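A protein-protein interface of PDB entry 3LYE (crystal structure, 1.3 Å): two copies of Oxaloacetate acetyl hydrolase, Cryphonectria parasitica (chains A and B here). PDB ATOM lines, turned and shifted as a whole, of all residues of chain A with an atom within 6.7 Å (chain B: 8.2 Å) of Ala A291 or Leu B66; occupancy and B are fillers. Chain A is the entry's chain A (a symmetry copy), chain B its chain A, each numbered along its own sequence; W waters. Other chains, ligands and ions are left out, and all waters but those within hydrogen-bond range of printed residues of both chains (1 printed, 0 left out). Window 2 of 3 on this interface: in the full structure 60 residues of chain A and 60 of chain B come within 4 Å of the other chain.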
ATOM      1  N   PHE A 283       7.199  20.787  14.031  1.00  0.00           N
ATOM      2  CA  PHE A 283       6.005  21.419  13.465  1.00  0.00           C
ATOM      3  C   PHE A 283       4.890  21.427  14.498  1.00  0.00           C
ATOM      4  O   PHE A 283       4.139  22.396  14.608  1.00  0.00           O
ATOM      5  CB  PHE A 283       5.555  20.744  12.189  1.00  0.00           C
ATOM      6  CG  PHE A 283       6.548  20.818  11.080  1.00  0.00           C
ATOM      7  CD1 PHE A 283       7.417  21.898  10.953  1.00  0.00           C
ATOM      8  CD2 PHE A 283       6.628  19.797  10.148  1.00  0.00           C
ATOM      9  CE1 PHE A 283       8.365  21.921   9.934  1.00  0.00           C
ATOM     10  CE2 PHE A 283       7.568  19.839   9.106  1.00  0.00           C
ATOM     11  CZ  PHE A 283       8.434  20.894   9.014  1.00  0.00           C
ATOM     12  N   GLY A 287       2.694  24.834  16.158  1.00  0.00           N
ATOM     13  CA  GLY A 287       1.330  25.023  15.703  1.00  0.00           C
ATOM     14  C   GLY A 287       0.735  24.204  14.604  1.00  0.00           C
ATOM     15  O   GLY A 287      -0.277  24.596  14.015  1.00  0.00           O
ATOM     16  N   LEU A 288       1.276  23.015  14.392  1.00  0.00           N
ATOM     17  CA  LEU A 288       0.736  22.180  13.324  1.00  0.00           C
ATOM     18  C   LEU A 288      -0.697  21.802  13.570  1.00  0.00           C
ATOM     19  O   LEU A 288      -1.503  21.834  12.651  1.00  0.00           O
ATOM     20  CB  LEU A 288       1.585  20.917  13.183  1.00  0.00           C
ATOM     21  CG  LEU A 288       1.091  19.939  12.109  1.00  0.00           C
ATOM     22  CD1 LEU A 288       1.166  20.558  10.741  1.00  0.00           C
ATOM     23  CD2 LEU A 288       1.956  18.672  12.170  1.00  0.00           C
ATOM     24  N   GLN A 289      -1.024  21.443  14.813  1.00  0.00           N
ATOM     25  CA  GLN A 289      -2.412  21.053  15.081  1.00  0.00           C
ATOM     26  C   GLN A 289      -3.398  22.181  14.785  1.00  0.00           C
ATOM     27  O   GLN A 289      -4.430  21.944  14.199  1.00  0.00           O
ATOM     28  CB  GLN A 289      -2.616  20.486  16.481  1.00  0.00           C
ATOM     29  CG  GLN A 289      -4.029  19.924  16.636  1.00  0.00           C
ATOM     30  CD  GLN A 289      -4.271  18.719  15.721  1.00  0.00           C
ATOM     31  OE1 GLN A 289      -3.381  17.892  15.519  1.00  0.00           O
ATOM     32  NE2 GLN A 289      -5.477  18.628  15.157  1.00  0.00           N
ATOM     33  N   ASP A 290      -3.075  23.415  15.126  1.00  0.00           N
ATOM     34  CA  ASP A 290      -3.984  24.516  14.839  1.00  0.00           C
ATOM     35  C   ASP A 290      -4.161  24.647  13.328  1.00  0.00           C
ATOM     36  O   ASP A 290      -5.258  24.904  12.825  1.00  0.00           O
ATOM     37  CB  ASP A 290      -3.387  25.846  15.305  1.00  0.00           C
ATOM     38  CG  ASP A 290      -3.487  26.059  16.789  1.00  0.00           C
ATOM     39  OD1 ASP A 290      -2.868  27.030  17.256  1.00  0.00           O
ATOM     40  OD2 ASP A 290      -4.193  25.302  17.488  1.00  0.00           O
ATOM     41  N   ALA A 291      -3.077  24.476  12.584  1.00  0.00           N
ATOM     42  CA  ALA A 291      -3.151  24.601  11.140  1.00  0.00           C
ATOM     43  C   ALA A 291      -3.967  23.488  10.520  1.00  0.00           C
ATOM     44  O   ALA A 291      -4.746  23.719   9.592  1.00  0.00           O
ATOM     45  CB  ALA A 291      -1.761  24.676  10.542  1.00  0.00           C
ATOM     46  N   MET A 292      -3.819  22.292  11.062  1.00  0.00           N
ATOM     47  CA  MET A 292      -4.556  21.145  10.551  1.00  0.00           C
ATOM     48  C   MET A 292      -6.045  21.332  10.828  1.00  0.00           C
ATOM     49  O   MET A 292      -6.875  20.935  10.034  1.00  0.00           O
ATOM     50  CB  MET A 292      -4.047  19.825  11.133  1.00  0.00           C
ATOM     51  CG  MET A 292      -2.669  19.408  10.651  1.00  0.00           C
ATOM     52  SD  MET A 292      -2.151  17.868  11.472  1.00  0.00           S
ATOM     53  CE  MET A 292      -0.964  17.173  10.302  1.00  0.00           C
ATOM     54  N   GLU A 293      -6.394  21.957  11.945  1.00  0.00           N
ATOM     55  CA  GLU A 293      -7.798  22.164  12.253  1.00  0.00           C
ATOM     56  C   GLU A 293      -8.387  23.180  11.290  1.00  0.00           C
ATOM     57  O   GLU A 293      -9.521  23.049  10.883  1.00  0.00           O
ATOM     58  CB  GLU A 293      -7.987  22.560  13.710  1.00  0.00           C
ATOM     59  CG  GLU A 293      -7.635  21.406  14.667  1.00  0.00           C
ATOM     60  CD  GLU A 293      -7.667  21.814  16.130  1.00  0.00           C
ATOM     61  OE1 GLU A 293      -7.511  20.915  16.996  1.00  0.00           O
ATOM     62  OE2 GLU A 293      -7.843  23.025  16.406  1.00  0.00           O
ATOM     63  N   VAL A 294      -7.613  24.189  10.921  1.00  0.00           N
ATOM     64  CA  VAL A 294      -8.106  25.181   9.984  1.00  0.00           C
ATOM     65  C   VAL A 294      -8.288  24.516   8.625  1.00  0.00           C
ATOM     66  O   VAL A 294      -9.328  24.652   7.991  1.00  0.00           O
ATOM     67  CB  VAL A 294      -7.085  26.340   9.789  1.00  0.00           C
ATOM     68  CG1 VAL A 294      -7.386  27.056   8.490  1.00  0.00           C
ATOM     69  CG2 VAL A 294      -7.105  27.277  10.987  1.00  0.00           C
ATOM     70  N   ASP A 295      -7.285  23.760   8.199  1.00  0.00           N
ATOM     71  CA  ASP A 295      -7.318  23.104   6.906  1.00  0.00           C
ATOM     72  C   ASP A 295      -8.462  22.106   6.804  1.00  0.00           C
ATOM     73  O   ASP A 295      -9.239  22.138   5.870  1.00  0.00           O
ATOM     74  CB  ASP A 295      -5.961  22.444   6.652  1.00  0.00           C
ATOM     75  CG  ASP A 295      -5.712  22.127   5.197  1.00  0.00           C
ATOM     76  OD1 ASP A 295      -5.321  20.979   4.934  1.00  0.00           O
ATOM     77  OD2 ASP A 295      -5.881  23.000   4.318  1.00  0.00           O
ATOM     78  N   ASN A 296      -8.595  21.253   7.799  1.00  0.00           N
ATOM     79  CA  ASN A 296      -9.635  20.258   7.802  1.00  0.00           C
ATOM     80  C   ASN A 296     -11.028  20.890   7.884  1.00  0.00           C
ATOM     81  O   ASN A 296     -11.952  20.467   7.174  1.00  0.00           O
ATOM     82  CB  ASN A 296      -9.403  19.269   8.955  1.00  0.00           C
ATOM     83  CG  ASN A 296      -8.169  18.370   8.746  1.00  0.00           C
ATOM     84  OD1 ASN A 296      -7.499  17.963   9.717  1.00  0.00           O
ATOM     85  ND2 ASN A 296      -7.876  18.038   7.487  1.00  0.00           N
ATOM     86  N   GLY B  53      13.769  26.885   4.821  1.00  0.00           N
ATOM     87  CA  GLY B  53      12.424  27.435   4.787  1.00  0.00           C
ATOM     88  C   GLY B  53      11.669  27.083   6.072  1.00  0.00           C
ATOM     89  O   GLY B  53      10.983  27.920   6.656  1.00  0.00           O
ATOM     90  N   ALA B  54      11.763  25.831   6.512  1.00  0.00           N
ATOM     91  CA  ALA B  54      11.078  25.408   7.730  1.00  0.00           C
ATOM     92  C   ALA B  54      11.610  26.189   8.911  1.00  0.00           C
ATOM     93  O   ALA B  54      10.859  26.551   9.790  1.00  0.00           O
ATOM     94  CB  ALA B  54      11.246  23.912   7.973  1.00  0.00           C
ATOM     95  N   THR B  57      10.433  29.782   8.850  1.00  0.00           N
ATOM     96  CA  THR B  57       9.043  29.828   9.254  1.00  0.00           C
ATOM     97  C   THR B  57       8.876  29.650  10.764  1.00  0.00           C
ATOM     98  O   THR B  57       8.128  30.392  11.413  1.00  0.00           O
ATOM     99  CB  THR B  57       8.212  28.785   8.491  1.00  0.00           C
ATOM    100  OG1 THR B  57       8.379  28.993   7.073  1.00  0.00           O
ATOM    101  CG2 THR B  57       6.753  28.961   8.776  1.00  0.00           C
ATOM    102  N   GLN B  63       5.459  29.280  13.066  1.00  0.00           N
ATOM    103  CA  GLN B  63       4.493  28.465  12.377  1.00  0.00           C
ATOM    104  C   GLN B  63       5.105  27.242  11.716  1.00  0.00           C
ATOM    105  O   GLN B  63       6.329  27.174  11.594  1.00  0.00           O
ATOM    106  CB  GLN B  63       3.810  29.324  11.306  1.00  0.00           C
ATOM    107  CG  GLN B  63       3.042  30.509  11.827  1.00  0.00           C
ATOM    108  CD  GLN B  63       1.848  30.185  12.653  1.00  0.00           C
ATOM    109  OE1 GLN B  63       1.454  30.947  13.590  1.00  0.00           O
ATOM    110  NE2 GLN B  63       1.221  29.103  12.326  1.00  0.00           N
ATOM    111  N   PRO B  64       4.270  26.251  11.370  1.00  0.00           N
ATOM    112  CA  PRO B  64       4.769  25.053  10.711  1.00  0.00           C
ATOM    113  C   PRO B  64       5.084  25.349   9.248  1.00  0.00           C
ATOM    114  O   PRO B  64       4.615  26.320   8.682  1.00  0.00           O
ATOM    115  CB  PRO B  64       3.607  24.082  10.785  1.00  0.00           C
ATOM    116  CG  PRO B  64       2.428  24.867  11.111  1.00  0.00           C
ATOM    117  CD  PRO B  64       2.823  26.203  11.600  1.00  0.00           C
ATOM    118  N   ASP B  65       5.792  24.423   8.613  1.00  0.00           N
ATOM    119  CA  ASP B  65       6.233  24.580   7.217  1.00  0.00           C
ATOM    120  C   ASP B  65       5.146  24.210   6.229  1.00  0.00           C
ATOM    121  O   ASP B  65       5.258  23.216   5.540  1.00  0.00           O
ATOM    122  CB  ASP B  65       7.490  23.705   7.050  1.00  0.00           C
ATOM    123  CG  ASP B  65       8.233  23.973   5.781  1.00  0.00           C
ATOM    124  OD1 ASP B  65       8.922  23.037   5.315  1.00  0.00           O
ATOM    125  OD2 ASP B  65       8.144  25.082   5.243  1.00  0.00           O
ATOM    126  N   LEU B  66       4.126  25.069   6.156  1.00  0.00           N
ATOM    127  CA  LEU B  66       2.960  24.867   5.305  1.00  0.00           C
ATOM    128  C   LEU B  66       2.664  26.049   4.377  1.00  0.00           C
ATOM    129  O   LEU B  66       1.547  26.543   4.287  1.00  0.00           O
ATOM    130  CB  LEU B  66       1.760  24.572   6.199  1.00  0.00           C
ATOM    131  CG  LEU B  66       1.860  23.284   7.020  1.00  0.00           C
ATOM    132  CD1 LEU B  66       0.760  23.188   8.049  1.00  0.00           C
ATOM    133  CD2 LEU B  66       1.811  22.097   6.081  1.00  0.00           C
ATOM    134  N   ALA B  67       3.694  26.537   3.710  1.00  0.00           N
ATOM    135  CA  ALA B  67       3.570  27.661   2.780  1.00  0.00           C
ATOM    136  C   ALA B  67       3.011  28.909   3.443  1.00  0.00           C
ATOM    137  O   ALA B  67       2.220  29.652   2.880  1.00  0.00           O
ATOM    138  CB  ALA B  67       2.747  27.283   1.566  1.00  0.00           C
ATOM    139  N   ILE B  68       3.463  29.139   4.669  1.00  0.00           N
ATOM    140  CA  ILE B  68       3.055  30.293   5.480  1.00  0.00           C
ATOM    141  C   ILE B  68       4.062  31.415   5.214  1.00  0.00           C
ATOM    142  O   ILE B  68       3.677  32.592   5.078  1.00  0.00           O
ATOM    143  CB  ILE B  68       2.861  29.910   6.941  1.00  0.00           C
ATOM    144  CG1 ILE B  68       1.644  28.965   7.050  1.00  0.00           C
ATOM    145  CG2 ILE B  68       2.675  31.146   7.776  1.00  0.00           C
ATOM    146  CD1 ILE B  68       1.502  28.261   8.362  1.00  0.00           C
ATOM    147  N   ALA B  69       5.348  31.109   5.205  1.00  0.00           N
ATOM    148  CA  ALA B  69       6.332  32.126   4.862  1.00  0.00           C
ATOM    149  C   ALA B  69       6.164  32.419   3.356  1.00  0.00           C
ATOM    150  O   ALA B  69       6.035  31.484   2.551  1.00  0.00           O
ATOM    151  CB  ALA B  69       7.722  31.647   5.145  1.00  0.00           C
ATOM    152  N   ASP B  96      11.474  27.789  -2.348  1.00  0.00           N
ATOM    153  CA  ASP B  96      10.223  27.066  -2.481  1.00  0.00           C
ATOM    154  C   ASP B  96       9.789  26.961  -3.959  1.00  0.00           C
ATOM    155  O   ASP B  96      10.564  26.427  -4.753  1.00  0.00           O
ATOM    156  CB  ASP B  96       9.191  27.726  -1.559  1.00  0.00           C
ATOM    157  CG  ASP B  96       9.574  27.613  -0.120  1.00  0.00           C
ATOM    158  OD1 ASP B  96       9.455  26.512   0.400  1.00  0.00           O
ATOM    159  OD2 ASP B  96      10.046  28.596   0.470  1.00  0.00           O
ATOM    160  N   LEU B 127       1.843  25.035  -5.185  1.00  0.00           N
ATOM    161  CA  LEU B 127       2.093  26.163  -4.303  1.00  0.00           C
ATOM    162  C   LEU B 127       1.094  26.287  -3.165  1.00  0.00           C
ATOM    163  O   LEU B 127       1.408  26.795  -2.085  1.00  0.00           O
ATOM    164  CB  LEU B 127       2.111  27.425  -5.163  1.00  0.00           C
ATOM    165  CG  LEU B 127       0.894  28.355  -5.257  1.00  0.00           C
ATOM    166  CD1 LEU B 127       1.237  29.606  -6.079  1.00  0.00           C
ATOM    167  CD2 LEU B 127      -0.265  27.647  -5.892  1.00  0.00           C
ATOM    168  N   THR B 128      -0.108  25.808  -3.436  1.00  0.00           N
ATOM    169  CA  THR B 128      -1.226  25.819  -2.514  1.00  0.00           C
ATOM    170  C   THR B 128      -1.036  24.865  -1.357  1.00  0.00           C
ATOM    171  O   THR B 128      -1.690  25.011  -0.326  1.00  0.00           O
ATOM    172  CB  THR B 128      -2.458  25.391  -3.292  1.00  0.00           C
ATOM    173  OG1 THR B 128      -2.264  25.717  -4.678  1.00  0.00           O
ATOM    174  CG2 THR B 128      -3.694  26.076  -2.769  1.00  0.00           C
HETATM  175  O   HOH W   1      -0.715  27.336  13.032  1.00  0.00           O
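Ala A291 touches just one residue of chain B: Leu B66 (3.8 Å).
Leu B66 touches two residues of chain A.
Of the printed residues of chain B, Gly A287 touches Pro B64.
Of the printed residues of chain B, Leu A288 touches Pro B64 (3.9 Å) and Leu B66 (3.8 Å).
Printed residues of chain A within 4 Å of Asp B65: Phe A283.
Of the printed residues of chain B, Phe A283 touches Asp B65.
Of the printed residues of chain A, Pro B64 touches Gly A287 (3.9 Å) and Leu A288 (3.9 Å).
Val A294 touches none of the printed residues of chain B.
Thr B128 touches none of the printed residues of chain A.
The nearest residue of chain A that does not touch Leu B66 is Met A292 (5.6 Å).
No position is printed for both chains.
Of the 5 pairs that touch across the chains among the printed residues, none has its exchanged pair printed and touching as well.
O of Phe A283 sits at hydrogen-bond distance from N of Leu A288 (2.9 Å).
CB of Asp B65 touches CE1 of Phe A283, 3.5 Å away.
C of Gly A287 touches CG of Pro B64, at 3.9 Å.
CG of Pro B64 touches CA of Leu A288, at 3.9 Å.
CD1 of Leu B66 touches CD1 of Leu A288, 3.8 Å away.
Ala A291 touches Leu B66 (CB to CD1, 3.8 Å).
Of the 13 printed residues of chain B, 3 touch a printed residue of chain A.
Hydrophobic or aromatic side chains of chain B within 4 Å of the printed part of chain A: Pro B64 and Leu B66.
Printed residues of chain A that touch a printed residue of chain B: Phe A283, Gly A287, Leu A288 and Ala A291.
Hydrophobic or aromatic side chains of chain A that line the printed part of chain B: Phe A283, Leu A288 and Ala A291.
Among the printed residues, 5 pairs touch across the chains.
Among the printed residues, no Asp or Glu carboxylate lies within 4 Å of a Lys or Arg side-chain nitrogen of the other chain.
Water W1 lies within hydrogen-bond range of the side-chain amide nitrogen (NE2) of Gln B63 (2.7 Å) and the backbone carbonyl oxygen (O) of Gly A287 (2.9 Å).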
